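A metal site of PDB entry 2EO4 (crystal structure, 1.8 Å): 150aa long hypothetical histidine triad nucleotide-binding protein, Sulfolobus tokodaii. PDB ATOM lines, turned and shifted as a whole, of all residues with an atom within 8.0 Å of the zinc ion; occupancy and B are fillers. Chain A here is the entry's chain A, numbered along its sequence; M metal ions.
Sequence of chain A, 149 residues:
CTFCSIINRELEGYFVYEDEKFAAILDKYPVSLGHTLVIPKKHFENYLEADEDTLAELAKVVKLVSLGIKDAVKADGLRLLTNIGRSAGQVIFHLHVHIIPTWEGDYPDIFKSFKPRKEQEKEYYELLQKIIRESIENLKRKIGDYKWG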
ATOM      1  N   CYS A   1       3.534  -1.500 -18.854  1.00  0.00           N
ATOM      2  CA  CYS A   1       4.708  -1.518 -19.771  1.00  0.00           C
ATOM      3  C   CYS A   1       4.241  -1.522 -21.224  1.00  0.00           C
ATOM      4  O   CYS A   1       3.439  -2.361 -21.620  1.00  0.00           O
ATOM      5  CB  CYS A   1       5.566  -2.753 -19.511  1.00  0.00           C
ATOM      6  SG  CYS A   1       6.939  -2.938 -20.688  1.00  0.00           S
ATOM      7  N   THR A   2       4.749  -0.581 -22.011  1.00  0.00           N
ATOM      8  CA  THR A   2       4.348  -0.485 -23.403  1.00  0.00           C
ATOM      9  C   THR A   2       4.630  -1.775 -24.198  1.00  0.00           C
ATOM     10  O   THR A   2       3.783  -2.214 -24.970  1.00  0.00           O
ATOM     11  CB  THR A   2       5.040   0.717 -24.088  1.00  0.00           C
ATOM     12  OG1 THR A   2       4.531   1.934 -23.529  1.00  0.00           O
ATOM     13  CG2 THR A   2       4.785   0.714 -25.587  1.00  0.00           C
ATOM     14  N   PHE A   3       5.810  -2.371 -24.013  1.00  0.00           N
ATOM     15  CA  PHE A   3       6.110  -3.585 -24.753  1.00  0.00           C
ATOM     16  C   PHE A   3       5.369  -4.829 -24.260  1.00  0.00           C
ATOM     17  O   PHE A   3       4.914  -5.640 -25.070  1.00  0.00           O
ATOM     18  CB  PHE A   3       7.620  -3.836 -24.809  1.00  0.00           C
ATOM     19  CG  PHE A   3       8.336  -2.901 -25.756  1.00  0.00           C
ATOM     20  CD1 PHE A   3       7.847  -2.704 -27.040  1.00  0.00           C
ATOM     21  CD2 PHE A   3       9.456  -2.196 -25.340  1.00  0.00           C
ATOM     22  CE1 PHE A   3       8.470  -1.809 -27.908  1.00  0.00           C
ATOM     23  CE2 PHE A   3      10.092  -1.300 -26.205  1.00  0.00           C
ATOM     24  CZ  PHE A   3       9.601  -1.101 -27.479  1.00  0.00           C
ATOM     25  N   CYS A   4       5.239  -4.974 -22.947  1.00  0.00           N
ATOM     26  CA  CYS A   4       4.492  -6.121 -22.429  1.00  0.00           C
ATOM     27  C   CYS A   4       3.056  -5.995 -22.949  1.00  0.00           C
ATOM     28  O   CYS A   4       2.422  -6.998 -23.290  1.00  0.00           O
ATOM     29  CB  CYS A   4       4.502  -6.130 -20.900  1.00  0.00           C
ATOM     30  SG  CYS A   4       6.037  -6.766 -20.151  1.00  0.00           S
ATOM     31  N   SER A   5       2.555  -4.762 -23.013  1.00  0.00           N
ATOM     32  CA  SER A   5       1.198  -4.520 -23.503  1.00  0.00           C
ATOM     33  C   SER A   5       1.046  -4.922 -24.966  1.00  0.00           C
ATOM     34  O   SER A   5       0.043  -5.517 -25.353  1.00  0.00           O
ATOM     35  CB  SER A   5       0.810  -3.048 -23.332  1.00  0.00           C
ATOM     36  OG  SER A   5       0.719  -2.695 -21.968  1.00  0.00           O
ATOM     37  N   ILE A   6       2.035  -4.592 -25.784  1.00  0.00           N
ATOM     38  CA  ILE A   6       1.976  -4.945 -27.192  1.00  0.00           C
ATOM     39  C   ILE A   6       2.067  -6.462 -27.349  1.00  0.00           C
ATOM     40  O   ILE A   6       1.390  -7.049 -28.184  1.00  0.00           O
ATOM     41  CB  ILE A   6       3.101  -4.230 -27.970  1.00  0.00           C
ATOM     42  CG1 ILE A   6       2.818  -2.724 -27.999  1.00  0.00           C
ATOM     43  CG2 ILE A   6       3.189  -4.779 -29.386  1.00  0.00           C
ATOM     44  CD1 ILE A   6       3.936  -1.875 -28.582  1.00  0.00           C
ATOM     45  N   ILE A   7       2.905  -7.085 -26.530  1.00  0.00           N
ATOM     46  CA  ILE A   7       3.065  -8.546 -26.588  1.00  0.00           C
ATOM     47  C   ILE A   7       1.735  -9.224 -26.256  1.00  0.00           C
ATOM     48  O   ILE A   7       1.356 -10.216 -26.885  1.00  0.00           O
ATOM     49  CB  ILE A   7       4.127  -9.026 -25.576  1.00  0.00           C
ATOM     50  CG1 ILE A   7       5.520  -8.560 -26.024  1.00  0.00           C
ATOM     51  CG2 ILE A   7       4.085 -10.543 -25.451  1.00  0.00           C
ATOM     52  CD1 ILE A   7       5.933  -9.091 -27.370  1.00  0.00           C
ATOM     53  N   ASN A   8       1.034  -8.679 -25.268  1.00  0.00           N
ATOM     54  CA  ASN A   8      -0.248  -9.244 -24.830  1.00  0.00           C
ATOM     55  C   ASN A   8      -1.442  -8.734 -25.638  1.00  0.00           C
ATOM     56  O   ASN A   8      -2.591  -9.025 -25.309  1.00  0.00           O
ATOM     57  CB  ASN A   8      -0.475  -8.948 -23.352  1.00  0.00           C
ATOM     58  CG  ASN A   8       0.561  -9.615 -22.460  1.00  0.00           C
ATOM     59  OD1 ASN A   8       0.878 -10.783 -22.645  1.00  0.00           O
ATOM     60  ND2 ASN A   8       1.073  -8.873 -21.481  1.00  0.00           N
ATOM     61  N   ILE A  39      12.682  -7.200 -29.081  1.00  0.00           N
ATOM     62  CA  ILE A  39      12.548  -7.360 -27.642  1.00  0.00           C
ATOM     63  C   ILE A  39      12.343  -8.785 -27.154  1.00  0.00           C
ATOM     64  O   ILE A  39      11.807  -9.634 -27.873  1.00  0.00           O
ATOM     65  CB  ILE A  39      11.325  -6.577 -27.111  1.00  0.00           C
ATOM     66  CG1 ILE A  39      10.041  -7.199 -27.671  1.00  0.00           C
ATOM     67  CG2 ILE A  39      11.413  -5.118 -27.537  1.00  0.00           C
ATOM     68  CD1 ILE A  39       8.770  -6.643 -27.071  1.00  0.00           C
ATOM     69  N   PRO A  40      12.791  -9.064 -25.919  1.00  0.00           N
ATOM     70  CA  PRO A  40      12.598 -10.395 -25.350  1.00  0.00           C
ATOM     71  C   PRO A  40      11.160 -10.223 -24.850  1.00  0.00           C
ATOM     72  O   PRO A  40      10.783  -9.101 -24.464  1.00  0.00           O
ATOM     73  CB  PRO A  40      13.576 -10.419 -24.172  1.00  0.00           C
ATOM     74  CG  PRO A  40      14.629  -9.401 -24.548  1.00  0.00           C
ATOM     75  CD  PRO A  40      13.796  -8.296 -25.154  1.00  0.00           C
ATOM     76  N   LYS A  41      10.353 -11.271 -24.870  1.00  0.00           N
ATOM     77  CA  LYS A  41       8.984 -11.133 -24.380  1.00  0.00           C
ATOM     78  C   LYS A  41       8.976 -10.951 -22.865  1.00  0.00           C
ATOM     79  O   LYS A  41       8.154 -10.216 -22.329  1.00  0.00           O
ATOM     80  CB  LYS A  41       8.143 -12.337 -24.798  1.00  0.00           C
ATOM     81  CG  LYS A  41       7.813 -12.340 -26.282  1.00  0.00           C
ATOM     82  CD  LYS A  41       6.875 -13.461 -26.652  1.00  0.00           C
ATOM     83  CE  LYS A  41       6.475 -13.363 -28.118  1.00  0.00           C
ATOM     84  NZ  LYS A  41       5.440 -14.385 -28.474  1.00  0.00           N
ATOM     85  N   LYS A  42       9.905 -11.623 -22.184  1.00  0.00           N
ATOM     86  CA  LYS A  42       9.995 -11.500 -20.741  1.00  0.00           C
ATOM     87  C   LYS A  42      10.485 -10.088 -20.415  1.00  0.00           C
ATOM     88  O   LYS A  42      11.364  -9.546 -21.096  1.00  0.00           O
ATOM     89  CB  LYS A  42      10.974 -12.518 -20.168  1.00  0.00           C
ATOM     90  CG  LYS A  42      11.153 -12.409 -18.662  1.00  0.00           C
ATOM     91  CD  LYS A  42      11.998 -13.536 -18.101  1.00  0.00           C
ATOM     92  CE  LYS A  42      12.140 -13.421 -16.593  1.00  0.00           C
ATOM     93  NZ  LYS A  42      12.930 -14.540 -16.016  1.00  0.00           N
ATOM     94  N   HIS A  43       9.922  -9.493 -19.373  1.00  0.00           N
ATOM     95  CA  HIS A  43      10.257  -8.134 -18.980  1.00  0.00           C
ATOM     96  C   HIS A  43      11.552  -7.999 -18.162  1.00  0.00           C
ATOM     97  O   HIS A  43      11.695  -8.577 -17.091  1.00  0.00           O
ATOM     98  CB  HIS A  43       9.098  -7.539 -18.175  1.00  0.00           C
ATOM     99  CG  HIS A  43       9.276  -6.092 -17.822  1.00  0.00           C
ATOM    100  ND1 HIS A  43       8.750  -5.067 -18.585  1.00  0.00           N
ATOM    101  CD2 HIS A  43       9.943  -5.502 -16.803  1.00  0.00           C
ATOM    102  CE1 HIS A  43       9.091  -3.904 -18.044  1.00  0.00           C
ATOM    103  NE2 HIS A  43       9.814  -4.141 -16.961  1.00  0.00           N
ATOM    104  N   PHE A  44      12.484  -7.215 -18.703  1.00  0.00           N
ATOM    105  CA  PHE A  44      13.758  -6.908 -18.052  1.00  0.00           C
ATOM    106  C   PHE A  44      13.879  -5.382 -18.181  1.00  0.00           C
ATOM    107  O   PHE A  44      13.620  -4.835 -19.242  1.00  0.00           O
ATOM    108  CB  PHE A  44      14.940  -7.568 -18.779  1.00  0.00           C
ATOM    109  CG  PHE A  44      14.979  -9.063 -18.630  1.00  0.00           C
ATOM    110  CD1 PHE A  44      15.271  -9.644 -17.401  1.00  0.00           C
ATOM    111  CD2 PHE A  44      14.730  -9.887 -19.724  1.00  0.00           C
ATOM    112  CE1 PHE A  44      15.326 -11.033 -17.265  1.00  0.00           C
ATOM    113  CE2 PHE A  44      14.774 -11.278 -19.601  1.00  0.00           C
ATOM    114  CZ  PHE A  44      15.076 -11.843 -18.362  1.00  0.00           C
ATOM    115  N   GLU A  45      14.257  -4.713 -17.095  1.00  0.00           N
ATOM    116  CA  GLU A  45      14.365  -3.259 -17.101  1.00  0.00           C
ATOM    117  C   GLU A  45      15.300  -2.726 -18.182  1.00  0.00           C
ATOM    118  O   GLU A  45      15.018  -1.695 -18.798  1.00  0.00           O
ATOM    119  CB  GLU A  45      14.849  -2.760 -15.735  1.00  0.00           C
ATOM    120  CG  GLU A  45      13.822  -2.906 -14.634  1.00  0.00           C
ATOM    121  CD  GLU A  45      12.599  -2.030 -14.854  1.00  0.00           C
ATOM    122  OE1 GLU A  45      12.757  -0.793 -14.917  1.00  0.00           O
ATOM    123  OE2 GLU A  45      11.492  -2.583 -14.971  1.00  0.00           O
ATOM    124  N   ILE A  92      11.625   3.673 -22.367  1.00  0.00           N
ATOM    125  CA  ILE A  92      10.752   2.517 -22.208  1.00  0.00           C
ATOM    126  C   ILE A  92      11.614   1.502 -21.465  1.00  0.00           C
ATOM    127  O   ILE A  92      12.605   0.991 -21.989  1.00  0.00           O
ATOM    128  CB  ILE A  92      10.295   1.900 -23.559  1.00  0.00           C
ATOM    129  CG1 ILE A  92       9.518   2.936 -24.369  1.00  0.00           C
ATOM    130  CG2 ILE A  92       9.403   0.690 -23.291  1.00  0.00           C
ATOM    131  CD1 ILE A  92       9.007   2.419 -25.707  1.00  0.00           C
ATOM    132  N   PHE A  93      11.229   1.212 -20.227  1.00  0.00           N
ATOM    133  CA  PHE A  93      12.013   0.316 -19.396  1.00  0.00           C
ATOM    134  C   PHE A  93      11.699  -1.166 -19.505  1.00  0.00           C
ATOM    135  O   PHE A  93      11.362  -1.836 -18.526  1.00  0.00           O
ATOM    136  CB  PHE A  93      11.965   0.828 -17.955  1.00  0.00           C
ATOM    137  CG  PHE A  93      12.549   2.203 -17.820  1.00  0.00           C
ATOM    138  CD1 PHE A  93      13.927   2.383 -17.717  1.00  0.00           C
ATOM    139  CD2 PHE A  93      11.741   3.336 -17.937  1.00  0.00           C
ATOM    140  CE1 PHE A  93      14.487   3.652 -17.736  1.00  0.00           C
ATOM    141  CE2 PHE A  93      12.291   4.612 -17.950  1.00  0.00           C
ATOM    142  CZ  PHE A  93      13.665   4.769 -17.854  1.00  0.00           C
ATOM    143  N   HIS A  94      11.823  -1.646 -20.737  1.00  0.00           N
ATOM    144  CA  HIS A  94      11.632  -3.040 -21.113  1.00  0.00           C
ATOM    145  C   HIS A  94      12.723  -3.179 -22.174  1.00  0.00           C
ATOM    146  O   HIS A  94      12.653  -2.520 -23.210  1.00  0.00           O
ATOM    147  CB  HIS A  94      10.266  -3.264 -21.767  1.00  0.00           C
ATOM    148  CG  HIS A  94      10.039  -4.676 -22.241  1.00  0.00           C
ATOM    149  ND1 HIS A  94       9.055  -5.494 -21.715  1.00  0.00           N
ATOM    150  CD2 HIS A  94      10.679  -5.423 -23.179  1.00  0.00           C
ATOM    151  CE1 HIS A  94       9.090  -6.665 -22.315  1.00  0.00           C
ATOM    152  NE2 HIS A  94      10.068  -6.644 -23.210  1.00  0.00           N
ATOM    153  N   LEU A  95      13.732  -4.001 -21.885  1.00  0.00           N
ATOM    154  CA  LEU A  95      14.853  -4.199 -22.795  1.00  0.00           C
ATOM    155  C   LEU A  95      14.470  -4.317 -24.263  1.00  0.00           C
ATOM    156  O   LEU A  95      13.688  -5.188 -24.638  1.00  0.00           O
ATOM    157  CB  LEU A  95      15.642  -5.445 -22.373  1.00  0.00           C
ATOM    158  CG  LEU A  95      16.742  -5.972 -23.306  1.00  0.00           C
ATOM    159  CD1 LEU A  95      17.752  -4.877 -23.642  1.00  0.00           C
ATOM    160  CD2 LEU A  95      17.432  -7.140 -22.618  1.00  0.00           C
HETATM  161 ZN    ZN M   1       7.636  -5.065 -20.236  1.00  0.00          ZN
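The backbone carbonyl oxygen (O) of Phe 93 lies close to a ring nitrogen (NE2) of His 43, 3.2 Å away.
OE2 of Glu 45 is in hydrogen-bond range of NE2 of His 43 (3.0 Å).
A ring nitrogen (NE2) of His 94 sits at hydrogen-bond distance from the backbone carbonyl oxygen (O) of Pro 40 (2.8 Å).
SG of Cys 1 sits close to N of Phe 3 (3.6 Å).
O of Cys 1 sits at hydrogen-bond distance from OG of Ser 5, 2.8 Å away.
The backbone carbonyl oxygen of Cys 4 lies within hydrogen-bond range of the side-chain amide nitrogen of Asn 8 (2.9 Å).
The zinc ion is bound by a ring nitrogen (ND1) of His 43, 2.0 Å away.
The zinc ion is bound by ND1 of His 94 (2.1 Å).
The zinc ion is bound by SG of Cys 1 (2.3 Å).
The zinc ion is bound by SG of Cys 4, 2.3 Å away.
The zinc ion has four donor atoms within binding distance.
Within 4 Å of the zinc ion: Cys 1, Cys 4, His 43 and His 94.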
